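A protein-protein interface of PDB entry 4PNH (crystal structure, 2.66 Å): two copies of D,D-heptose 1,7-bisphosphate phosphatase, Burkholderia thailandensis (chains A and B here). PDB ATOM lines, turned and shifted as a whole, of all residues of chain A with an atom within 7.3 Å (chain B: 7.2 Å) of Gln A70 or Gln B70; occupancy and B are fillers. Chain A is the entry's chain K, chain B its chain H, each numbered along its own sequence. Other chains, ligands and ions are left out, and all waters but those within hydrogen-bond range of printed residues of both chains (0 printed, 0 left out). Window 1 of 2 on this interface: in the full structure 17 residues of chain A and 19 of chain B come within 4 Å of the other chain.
OE1 of Gln A70 is in hydrogen-bond range of NE2 of Gln B70 (2.9 Å).
The backbone carbonyl oxygen of Phe A105 lies close to the backbone carbonyl oxygen of Gly B76, at 3.2 Å.
SG of Cys B107 lies close to NE2 of Gln A70 (3.8 Å).
The backbone carbonyl oxygen of Gly A76 lies close to the backbone carbonyl oxygen of Phe B105 (2.8 Å).
The side-chain sulfur (SG) of Cys B107 is disulfide-bonded to the side-chain sulfur (SG) of Cys A107.
N of Phe B105 is in hydrogen-bond range of O of Phe A78 (2.9 Å).
The backbone carbonyl oxygen (O) of Phe B78 is in hydrogen-bond range of the backbone NH (N) of Phe A105 (3.5 Å).
The backbone carbonyl oxygen (O) of Thr B68 is in hydrogen-bond range of the backbone NH (N) of Phe B106 (2.8 Å).
The backbone NH of Phe A106 sits at hydrogen-bond distance from the backbone carbonyl oxygen of Thr A68 (3.0 Å).
The side-chain sulfur (SG) of Cys A107 sits close to the side-chain amide nitrogen (NE2) of Gln A70 (3.7 Å).
The backbone carbonyl oxygen (O) of Phe A106 lies within hydrogen-bond range of the backbone NH (N) of Gln A70, at 2.9 Å.
The backbone NH of Thr A68 sits at hydrogen-bond distance from the backbone carbonyl oxygen of Val A104.
N of Gln B70 lies within hydrogen-bond range of O of Phe B106 (2.6 Å).
Among the printed residues, pairs that only touch across the chains: Phe A78 with Gln B70, Gly A76 with Phe B106, Gly A76 with Cys B107, Cys A107 with Gln B70, Gln A70 with Phe B78, Leu A83 with Leu B83, Arg A75 with Phe B106, Cys A107 with Gly B76, Val A104 with Phe B78, Cys A107 with Ser B71, Phe A106 with Gly B76 and Arg A75 with Cys B107.
Gln A70 touches just these residues of chain B: Gln B70 (2.9 Å), Phe B78 (3.5 Å) and Cys B107 (3.4 Å).
Of chain A, only Gln A70 (2.9 Å), Phe A78 (3.1 Å) and Cys A107 (3.4 Å) come within 4 Å of Gln B70.
Of the printed residues of chain A, Phe B106 touches Arg A75 (3.7 Å) and Gly A76 (3.1 Å).
Of the printed residues of chain B, Gly A76 touches Phe B105, Phe B106 and Cys B107.
Of the printed residues of chain B, Arg A75 touches Phe B106 and Cys B107.
Ile A73 touches none of the printed residues of chain B.
The nearest residue of chain A that does not touch Gln B70 is Leu A83 (4.4 Å).
Hydrophobic or aromatic side chains of chain A within 4 Å of the printed part of chain B: Phe A78, Leu A83 and Phe A105.
Printed residues of chain B that touch a printed residue of chain A: Gln B70, Ser B71, Gly B76, Phe B78, Leu B83, Phe B105, Phe B106 and Cys B107.
Among the printed residues, 19 pairs touch across the chains.
Gln A70 touches Phe B78, and with the chains exchanged Phe A78 touches Gln B70.
Gly A76 touches Phe B106, and with the chains exchanged Phe A106 touches Gly B76.
Phe A78 touches Phe B105, and with the chains exchanged Phe A105 touches Phe B78.
Cys B107 touches its own counterpart, Cys A107.
Positions printed for both chains: 67, 68, 69, 70, 71, 72, 73, 74, 75, 76, 78, 83, 105, 106, 107 and 124.
Of the 19 pairs that touch across the chains among the printed residues, 15 have their exchanged pair printed and touching as well.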
ATOM      1  N   ASP A  27      17.596   5.592   5.030  1.00  0.00           N
ATOM      2  CA  ASP A  27      16.487   5.240   4.151  1.00  0.00           C
ATOM      3  C   ASP A  27      16.811   5.493   2.690  1.00  0.00           C
ATOM      4  O   ASP A  27      17.282   6.569   2.335  1.00  0.00           O
ATOM      5  CB  ASP A  27      15.227   6.018   4.538  1.00  0.00           C
ATOM      6  CG  ASP A  27      14.594   5.509   5.819  1.00  0.00           C
ATOM      7  OD1 ASP A  27      14.690   4.294   6.092  1.00  0.00           O
ATOM      8  OD2 ASP A  27      14.014   6.330   6.561  1.00  0.00           O
ATOM      9  N   ALA A  67      23.435   8.181   9.252  1.00  0.00           N
ATOM     10  CA  ALA A  67      22.488   9.035   9.939  1.00  0.00           C
ATOM     11  C   ALA A  67      21.077   8.536   9.670  1.00  0.00           C
ATOM     12  O   ALA A  67      20.629   8.491   8.524  1.00  0.00           O
ATOM     13  CB  ALA A  67      22.648  10.478   9.495  1.00  0.00           C
ATOM     14  N   THR A  68      20.388   8.143  10.736  1.00  0.00           N
ATOM     15  CA  THR A  68      19.019   7.657  10.629  1.00  0.00           C
ATOM     16  C   THR A  68      18.044   8.734  11.098  1.00  0.00           C
ATOM     17  O   THR A  68      17.987   9.068  12.281  1.00  0.00           O
ATOM     18  CB  THR A  68      18.809   6.374  11.457  1.00  0.00           C
ATOM     19  OG1 THR A  68      19.857   5.437  11.170  1.00  0.00           O
ATOM     20  CG2 THR A  68      17.468   5.744  11.134  1.00  0.00           C
ATOM     21  N   ASN A  69      17.280   9.275  10.153  1.00  0.00           N
ATOM     22  CA  ASN A  69      16.295  10.307  10.448  1.00  0.00           C
ATOM     23  C   ASN A  69      15.072   9.710  11.144  1.00  0.00           C
ATOM     24  O   ASN A  69      14.263   9.015  10.521  1.00  0.00           O
ATOM     25  CB  ASN A  69      15.904  11.029   9.150  1.00  0.00           C
ATOM     26  CG  ASN A  69      15.071  12.274   9.392  1.00  0.00           C
ATOM     27  OD1 ASN A  69      15.611  13.378   9.504  1.00  0.00           O
ATOM     28  ND2 ASN A  69      13.756  12.111   9.449  1.00  0.00           N
ATOM     29  N   GLN A  70      14.957   9.972  12.444  1.00  0.00           N
ATOM     30  CA  GLN A  70      13.930   9.354  13.295  1.00  0.00           C
ATOM     31  C   GLN A  70      12.482   9.726  12.988  1.00  0.00           C
ATOM     32  O   GLN A  70      11.565   9.048  13.451  1.00  0.00           O
ATOM     33  CB  GLN A  70      14.195   9.677  14.763  1.00  0.00           C
ATOM     34  CG  GLN A  70      14.665   8.496  15.579  1.00  0.00           C
ATOM     35  CD  GLN A  70      15.232   8.904  16.915  1.00  0.00           C
ATOM     36  OE1 GLN A  70      15.722   8.070  17.673  1.00  0.00           O
ATOM     37  NE2 GLN A  70      15.156  10.192  17.220  1.00  0.00           N
ATOM     38  N   SER A  71      12.255  10.797  12.233  1.00  0.00           N
ATOM     39  CA  SER A  71      10.883  11.162  11.867  1.00  0.00           C
ATOM     40  C   SER A  71      10.208  10.031  11.091  1.00  0.00           C
ATOM     41  O   SER A  71       8.981   9.948  11.032  1.00  0.00           O
ATOM     42  CB  SER A  71      10.834  12.553  11.230  1.00  0.00           C
ATOM     43  OG  SER A  71       9.488  12.945  11.000  1.00  0.00           O
ATOM     44  N   GLY A  72      11.026   9.167  10.498  1.00  0.00           N
ATOM     45  CA  GLY A  72      10.547   8.005   9.782  1.00  0.00           C
ATOM     46  C   GLY A  72      10.623   6.687  10.532  1.00  0.00           C
ATOM     47  O   GLY A  72      10.942   5.652   9.946  1.00  0.00           O
ATOM     48  N   ILE A  73      10.280   6.720  11.816  1.00  0.00           N
ATOM     49  CA  ILE A  73      10.243   5.510  12.629  1.00  0.00           C
ATOM     50  C   ILE A  73       8.813   5.123  13.009  1.00  0.00           C
ATOM     51  O   ILE A  73       8.575   4.601  14.098  1.00  0.00           O
ATOM     52  CB  ILE A  73      11.080   5.668  13.913  1.00  0.00           C
ATOM     53  CG1 ILE A  73      12.524   6.032  13.567  1.00  0.00           C
ATOM     54  CG2 ILE A  73      11.030   4.393  14.741  1.00  0.00           C
ATOM     55  CD1 ILE A  73      13.219   5.011  12.693  1.00  0.00           C
ATOM     56  N   GLY A  74       7.866   5.379  12.110  1.00  0.00           N
ATOM     57  CA  GLY A  74       6.475   5.033  12.355  1.00  0.00           C
ATOM     58  C   GLY A  74       5.790   6.085  13.210  1.00  0.00           C
ATOM     59  O   GLY A  74       4.879   5.758  13.970  1.00  0.00           O
ATOM     60  N   ARG A  75       6.236   7.333  13.101  1.00  0.00           N
ATOM     61  CA  ARG A  75       5.688   8.456  13.871  1.00  0.00           C
ATOM     62  C   ARG A  75       5.900   8.278  15.378  1.00  0.00           C
ATOM     63  O   ARG A  75       4.971   8.441  16.164  1.00  0.00           O
ATOM     64  CB  ARG A  75       4.194   8.660  13.577  1.00  0.00           C
ATOM     65  CG  ARG A  75       3.881   9.213  12.196  1.00  0.00           C
ATOM     66  CD  ARG A  75       2.380   9.414  12.020  1.00  0.00           C
ATOM     67  NE  ARG A  75       1.761  10.001  13.207  1.00  0.00           N
ATOM     68  CZ  ARG A  75       0.492  10.394  13.273  1.00  0.00           C
ATOM     69  NH1 ARG A  75      -0.301  10.266  12.218  1.00  0.00           N
ATOM     70  NH2 ARG A  75       0.016  10.916  14.395  1.00  0.00           N
ATOM     71  N   GLY A  76       7.124   7.935  15.769  1.00  0.00           N
ATOM     72  CA  GLY A  76       7.510   7.906  17.169  1.00  0.00           C
ATOM     73  C   GLY A  76       6.896   6.898  18.131  1.00  0.00           C
ATOM     74  O   GLY A  76       6.823   7.179  19.327  1.00  0.00           O
ATOM     75  N   PHE A  78       7.682   3.502  19.712  1.00  0.00           N
ATOM     76  CA  PHE A  78       8.631   2.403  19.869  1.00  0.00           C
ATOM     77  C   PHE A  78       9.191   2.259  21.279  1.00  0.00           C
ATOM     78  O   PHE A  78       9.446   3.247  21.971  1.00  0.00           O
ATOM     79  CB  PHE A  78       9.791   2.554  18.880  1.00  0.00           C
ATOM     80  CG  PHE A  78      10.404   3.923  18.863  1.00  0.00           C
ATOM     81  CD1 PHE A  78      11.540   4.194  19.604  1.00  0.00           C
ATOM     82  CD2 PHE A  78       9.850   4.937  18.097  1.00  0.00           C
ATOM     83  CE1 PHE A  78      12.107   5.450  19.583  1.00  0.00           C
ATOM     84  CE2 PHE A  78      10.412   6.195  18.075  1.00  0.00           C
ATOM     85  CZ  PHE A  78      11.541   6.453  18.818  1.00  0.00           C
ATOM     86  N   LEU A  83      14.172  -0.649  18.788  1.00  0.00           N
ATOM     87  CA  LEU A  83      15.394   0.084  18.477  1.00  0.00           C
ATOM     88  C   LEU A  83      16.640  -0.794  18.429  1.00  0.00           C
ATOM     89  O   LEU A  83      17.477  -0.640  17.542  1.00  0.00           O
ATOM     90  CB  LEU A  83      15.595   1.202  19.497  1.00  0.00           C
ATOM     91  CG  LEU A  83      15.394   2.621  18.970  1.00  0.00           C
ATOM     92  CD1 LEU A  83      15.444   3.608  20.115  1.00  0.00           C
ATOM     93  CD2 LEU A  83      16.460   2.943  17.931  1.00  0.00           C
ATOM     94  N   VAL A 104      24.216   6.733  14.106  1.00  0.00           N
ATOM     95  CA  VAL A 104      23.627   7.852  14.826  1.00  0.00           C
ATOM     96  C   VAL A 104      22.153   8.007  14.459  1.00  0.00           C
ATOM     97  O   VAL A 104      21.730   7.621  13.367  1.00  0.00           O
ATOM     98  CB  VAL A 104      24.364   9.174  14.534  1.00  0.00           C
ATOM     99  CG1 VAL A 104      25.806   9.097  15.015  1.00  0.00           C
ATOM    100  CG2 VAL A 104      24.310   9.500  13.047  1.00  0.00           C
ATOM    101  N   PHE A 105      21.377   8.567  15.382  1.00  0.00           N
ATOM    102  CA  PHE A 105      19.935   8.707  15.214  1.00  0.00           C
ATOM    103  C   PHE A 105      19.532  10.147  15.526  1.00  0.00           C
ATOM    104  O   PHE A 105      19.962  10.711  16.532  1.00  0.00           O
ATOM    105  CB  PHE A 105      19.171   7.726  16.112  1.00  0.00           C
ATOM    106  CG  PHE A 105      19.449   6.275  15.812  1.00  0.00           C
ATOM    107  CD1 PHE A 105      18.764   5.615  14.802  1.00  0.00           C
ATOM    108  CD2 PHE A 105      20.383   5.565  16.551  1.00  0.00           C
ATOM    109  CE1 PHE A 105      19.014   4.280  14.524  1.00  0.00           C
ATOM    110  CE2 PHE A 105      20.636   4.231  16.281  1.00  0.00           C
ATOM    111  CZ  PHE A 105      19.949   3.588  15.266  1.00  0.00           C
ATOM    112  N   PHE A 106      18.722  10.749  14.661  1.00  0.00           N
ATOM    113  CA  PHE A 106      18.421  12.172  14.789  1.00  0.00           C
ATOM    114  C   PHE A 106      16.941  12.454  14.986  1.00  0.00           C
ATOM    115  O   PHE A 106      16.100  11.863  14.322  1.00  0.00           O
ATOM    116  CB  PHE A 106      18.917  12.928  13.554  1.00  0.00           C
ATOM    117  CG  PHE A 106      18.427  14.348  13.476  1.00  0.00           C
ATOM    118  CD1 PHE A 106      18.982  15.333  14.277  1.00  0.00           C
ATOM    119  CD2 PHE A 106      17.410  14.697  12.600  1.00  0.00           C
ATOM    120  CE1 PHE A 106      18.531  16.640  14.209  1.00  0.00           C
ATOM    121  CE2 PHE A 106      16.956  16.001  12.529  1.00  0.00           C
ATOM    122  CZ  PHE A 106      17.518  16.972  13.334  1.00  0.00           C
ATOM    123  N   CYS A 107      16.631  13.363  15.904  1.00  0.00           N
ATOM    124  CA  CYS A 107      15.247  13.725  16.188  1.00  0.00           C
ATOM    125  C   CYS A 107      15.102  15.230  16.391  1.00  0.00           C
ATOM    126  O   CYS A 107      14.478  15.918  15.584  1.00  0.00           O
ATOM    127  CB  CYS A 107      14.741  12.977  17.422  1.00  0.00           C
ATOM    128  SG  CYS A 107      12.977  13.195  17.755  1.00  0.00           S
ATOM    129  N   MET A 124      20.805  18.135  12.438  1.00  0.00           N
ATOM    130  CA  MET A 124      21.547  16.887  12.277  1.00  0.00           C
ATOM    131  C   MET A 124      22.970  17.149  11.778  1.00  0.00           C
ATOM    132  O   MET A 124      23.921  16.998  12.544  1.00  0.00           O
ATOM    133  CB  MET A 124      20.792  15.939  11.341  1.00  0.00           C
ATOM    134  CG  MET A 124      21.377  14.534  11.235  1.00  0.00           C
ATOM    135  SD  MET A 124      20.343  13.420  10.243  1.00  0.00           S
ATOM    136  CE  MET A 124      20.851  13.754   8.561  1.00  0.00           C
ATOM    137  N   ALA B  67       6.242   8.075  28.781  1.00  0.00           N
ATOM    138  CA  ALA B  67       6.387   8.645  27.459  1.00  0.00           C
ATOM    139  C   ALA B  67       7.524   9.657  27.417  1.00  0.00           C
ATOM    140  O   ALA B  67       7.457  10.709  28.055  1.00  0.00           O
ATOM    141  CB  ALA B  67       5.097   9.285  27.043  1.00  0.00           C
ATOM    142  N   THR B  68       8.563   9.330  26.654  1.00  0.00           N
ATOM    143  CA  THR B  68       9.717  10.208  26.493  1.00  0.00           C
ATOM    144  C   THR B  68       9.789  10.874  25.118  1.00  0.00           C
ATOM    145  O   THR B  68       9.995  10.209  24.104  1.00  0.00           O
ATOM    146  CB  THR B  68      11.040   9.460  26.738  1.00  0.00           C
ATOM    147  OG1 THR B  68      10.966   8.747  27.978  1.00  0.00           O
ATOM    148  CG2 THR B  68      12.193  10.448  26.806  1.00  0.00           C
ATOM    149  N   ASN B  69       9.631  12.191  25.099  1.00  0.00           N
ATOM    150  CA  ASN B  69       9.765  12.969  23.873  1.00  0.00           C
ATOM    151  C   ASN B  69      11.216  13.041  23.418  1.00  0.00           C
ATOM    152  O   ASN B  69      12.044  13.665  24.073  1.00  0.00           O
ATOM    153  CB  ASN B  69       9.221  14.391  24.061  1.00  0.00           C
ATOM    154  CG  ASN B  69       7.713  14.434  24.210  1.00  0.00           C
ATOM    155  OD1 ASN B  69       6.988  14.600  23.225  1.00  0.00           O
ATOM    156  ND2 ASN B  69       7.228  14.262  25.435  1.00  0.00           N
ATOM    157  N   GLN B  70      11.524  12.376  22.306  1.00  0.00           N
ATOM    158  CA  GLN B  70      12.897  12.286  21.808  1.00  0.00           C
ATOM    159  C   GLN B  70      13.418  13.672  21.459  1.00  0.00           C
ATOM    160  O   GLN B  70      14.613  13.866  21.238  1.00  0.00           O
ATOM    161  CB  GLN B  70      12.994  11.359  20.599  1.00  0.00           C
ATOM    162  CG  GLN B  70      13.739  10.071  20.893  1.00  0.00           C
ATOM    163  CD  GLN B  70      13.544   9.014  19.825  1.00  0.00           C
ATOM    164  OE1 GLN B  70      12.886   9.250  18.811  1.00  0.00           O
ATOM    165  NE2 GLN B  70      14.114   7.836  20.053  1.00  0.00           N
ATOM    166  N   SER B  71      12.501  14.634  21.399  1.00  0.00           N
ATOM    167  CA  SER B  71      12.855  16.029  21.187  1.00  0.00           C
ATOM    168  C   SER B  71      13.639  16.573  22.387  1.00  0.00           C
ATOM    169  O   SER B  71      14.032  17.742  22.409  1.00  0.00           O
ATOM    170  CB  SER B  71      11.593  16.867  20.966  1.00  0.00           C
ATOM    171  OG  SER B  71      10.831  16.358  19.886  1.00  0.00           O
ATOM    172  N   GLY B  72      13.840  15.729  23.395  1.00  0.00           N
ATOM    173  CA  GLY B  72      14.611  16.104  24.562  1.00  0.00           C
ATOM    174  C   GLY B  72      15.927  15.392  24.818  1.00  0.00           C
ATOM    175  O   GLY B  72      16.539  15.599  25.867  1.00  0.00           O
ATOM    176  N   ILE B  73      16.367  14.576  23.870  1.00  0.00           N
ATOM    177  CA  ILE B  73      17.674  13.939  23.957  1.00  0.00           C
ATOM    178  C   ILE B  73      18.863  14.751  23.464  1.00  0.00           C
ATOM    179  O   ILE B  73      19.464  14.429  22.439  1.00  0.00           O
ATOM    180  CB  ILE B  73      17.601  12.616  23.176  1.00  0.00           C
ATOM    181  CG1 ILE B  73      16.248  11.938  23.399  1.00  0.00           C
ATOM    182  CG2 ILE B  73      18.739  11.692  23.584  1.00  0.00           C
ATOM    183  CD1 ILE B  73      16.219  10.481  22.988  1.00  0.00           C
ATOM    184  N   GLY B  74      19.192  15.814  24.191  1.00  0.00           N
ATOM    185  CA  GLY B  74      20.197  16.754  23.730  1.00  0.00           C
ATOM    186  C   GLY B  74      20.134  17.108  22.256  1.00  0.00           C
ATOM    187  O   GLY B  74      21.159  17.122  21.578  1.00  0.00           O
ATOM    188  N   ARG B  75      18.925  17.378  21.768  1.00  0.00           N
ATOM    189  CA  ARG B  75      18.687  17.735  20.367  1.00  0.00           C
ATOM    190  C   ARG B  75      19.260  16.730  19.366  1.00  0.00           C
ATOM    191  O   ARG B  75      20.041  17.096  18.495  1.00  0.00           O
ATOM    192  CB  ARG B  75      19.263  19.131  20.104  1.00  0.00           C
ATOM    193  CG  ARG B  75      18.495  20.252  20.779  1.00  0.00           C
ATOM    194  CD  ARG B  75      19.088  21.608  20.437  1.00  0.00           C
ATOM    195  NE  ARG B  75      20.433  21.770  20.981  1.00  0.00           N
ATOM    196  CZ  ARG B  75      21.201  22.835  20.778  1.00  0.00           C
ATOM    197  NH1 ARG B  75      20.762  23.843  20.035  1.00  0.00           N
ATOM    198  NH2 ARG B  75      22.411  22.894  21.318  1.00  0.00           N
ATOM    199  N   GLY B  76      18.878  15.464  19.501  1.00  0.00           N
ATOM    200  CA  GLY B  76      19.232  14.437  18.535  1.00  0.00           C
ATOM    201  C   GLY B  76      20.696  14.052  18.387  1.00  0.00           C
ATOM    202  O   GLY B  76      21.111  13.578  17.328  1.00  0.00           O
ATOM    203  N   LEU B  77      21.489  14.240  19.437  1.00  0.00           N
ATOM    204  CA  LEU B  77      22.878  13.809  19.379  1.00  0.00           C
ATOM    205  C   LEU B  77      23.065  12.598  20.295  1.00  0.00           C
ATOM    206  O   LEU B  77      23.232  12.726  21.505  1.00  0.00           O
ATOM    207  CB  LEU B  77      23.830  14.975  19.733  1.00  0.00           C
ATOM    208  CG  LEU B  77      24.011  15.637  21.111  1.00  0.00           C
ATOM    209  CD1 LEU B  77      25.157  15.017  21.899  1.00  0.00           C
ATOM    210  CD2 LEU B  77      24.232  17.135  20.961  1.00  0.00           C
ATOM    211  N   PHE B  78      22.985  11.407  19.708  1.00  0.00           N
ATOM    212  CA  PHE B  78      23.139  10.185  20.486  1.00  0.00           C
ATOM    213  C   PHE B  78      23.401   8.961  19.620  1.00  0.00           C
ATOM    214  O   PHE B  78      22.834   8.814  18.536  1.00  0.00           O
ATOM    215  CB  PHE B  78      21.896   9.913  21.345  1.00  0.00           C
ATOM    216  CG  PHE B  78      20.597   9.951  20.583  1.00  0.00           C
ATOM    217  CD1 PHE B  78      19.955   8.773  20.243  1.00  0.00           C
ATOM    218  CD2 PHE B  78      20.023  11.153  20.199  1.00  0.00           C
ATOM    219  CE1 PHE B  78      18.764   8.790  19.542  1.00  0.00           C
ATOM    220  CE2 PHE B  78      18.831  11.176  19.499  1.00  0.00           C
ATOM    221  CZ  PHE B  78      18.201   9.994  19.169  1.00  0.00           C
ATOM    222  N   LEU B  83      21.420   6.007  24.408  1.00  0.00           N
ATOM    223  CA  LEU B  83      20.027   5.604  24.547  1.00  0.00           C
ATOM    224  C   LEU B  83      19.854   4.486  25.568  1.00  0.00           C
ATOM    225  O   LEU B  83      18.921   4.507  26.370  1.00  0.00           O
ATOM    226  CB  LEU B  83      19.480   5.169  23.186  1.00  0.00           C
ATOM    227  CG  LEU B  83      18.468   6.101  22.521  1.00  0.00           C
ATOM    228  CD1 LEU B  83      18.173   5.624  21.114  1.00  0.00           C
ATOM    229  CD2 LEU B  83      17.191   6.161  23.344  1.00  0.00           C
ATOM    230  N   MET B  86      20.199   5.540  29.381  1.00  0.00           N
ATOM    231  CA  MET B  86      19.015   6.188  29.930  1.00  0.00           C
ATOM    232  C   MET B  86      17.906   5.208  30.288  1.00  0.00           C
ATOM    233  O   MET B  86      17.295   5.326  31.347  1.00  0.00           O
ATOM    234  CB  MET B  86      18.475   7.220  28.941  1.00  0.00           C
ATOM    235  CG  MET B  86      17.143   7.837  29.345  1.00  0.00           C
ATOM    236  SD  MET B  86      16.459   8.918  28.075  1.00  0.00           S
ATOM    237  CE  MET B  86      16.205   7.736  26.757  1.00  0.00           C
ATOM    238  N   PHE B 105       9.195   5.707  23.509  1.00  0.00           N
ATOM    239  CA  PHE B 105      10.012   6.842  23.089  1.00  0.00           C
ATOM    240  C   PHE B 105       9.383   7.469  21.845  1.00  0.00           C
ATOM    241  O   PHE B 105       9.070   6.755  20.893  1.00  0.00           O
ATOM    242  CB  PHE B 105      11.453   6.392  22.826  1.00  0.00           C
ATOM    243  CG  PHE B 105      12.120   5.781  24.027  1.00  0.00           C
ATOM    244  CD1 PHE B 105      12.717   6.576  24.989  1.00  0.00           C
ATOM    245  CD2 PHE B 105      12.124   4.407  24.207  1.00  0.00           C
ATOM    246  CE1 PHE B 105      13.314   6.013  26.102  1.00  0.00           C
ATOM    247  CE2 PHE B 105      12.722   3.835  25.320  1.00  0.00           C
ATOM    248  CZ  PHE B 105      13.318   4.640  26.267  1.00  0.00           C
ATOM    249  N   PHE B 106       9.212   8.791  21.840  1.00  0.00           N
ATOM    250  CA  PHE B 106       8.437   9.444  20.782  1.00  0.00           C
ATOM    251  C   PHE B 106       9.233  10.467  19.968  1.00  0.00           C
ATOM    252  O   PHE B 106      10.015  11.228  20.522  1.00  0.00           O
ATOM    253  CB  PHE B 106       7.215  10.120  21.399  1.00  0.00           C
ATOM    254  CG  PHE B 106       6.461  10.991  20.442  1.00  0.00           C
ATOM    255  CD1 PHE B 106       5.630  10.424  19.499  1.00  0.00           C
ATOM    256  CD2 PHE B 106       6.586  12.372  20.476  1.00  0.00           C
ATOM    257  CE1 PHE B 106       4.932  11.215  18.598  1.00  0.00           C
ATOM    258  CE2 PHE B 106       5.912  13.166  19.576  1.00  0.00           C
ATOM    259  CZ  PHE B 106       5.073  12.590  18.638  1.00  0.00           C
ATOM    260  N   CYS B 107       9.023  10.472  18.656  1.00  0.00           N
ATOM    261  CA  CYS B 107       9.718  11.398  17.771  1.00  0.00           C
ATOM    262  C   CYS B 107       8.781  11.949  16.702  1.00  0.00           C
ATOM    263  O   CYS B 107       7.592  11.628  16.679  1.00  0.00           O
ATOM    264  CB  CYS B 107      10.918  10.713  17.114  1.00  0.00           C
ATOM    265  SG  CYS B 107      11.953  11.811  16.118  1.00  0.00           S
ATOM    266  N   MET B 124       1.549  11.411  19.674  1.00  0.00           N
ATOM    267  CA  MET B 124       1.950  10.462  20.699  1.00  0.00           C
ATOM    268  C   MET B 124       0.784   9.647  21.226  1.00  0.00           C
ATOM    269  O   MET B 124       0.665   8.453  20.965  1.00  0.00           O
ATOM    270  CB  MET B 124       2.570  11.174  21.890  1.00  0.00           C
ATOM    271  CG  MET B 124       3.153  10.194  22.906  1.00  0.00           C
ATOM    272  SD  MET B 124       3.789  10.975  24.405  1.00  0.00           S
ATOM    273  CE  MET B 124       5.140  11.937  23.841  1.00  0.00           C
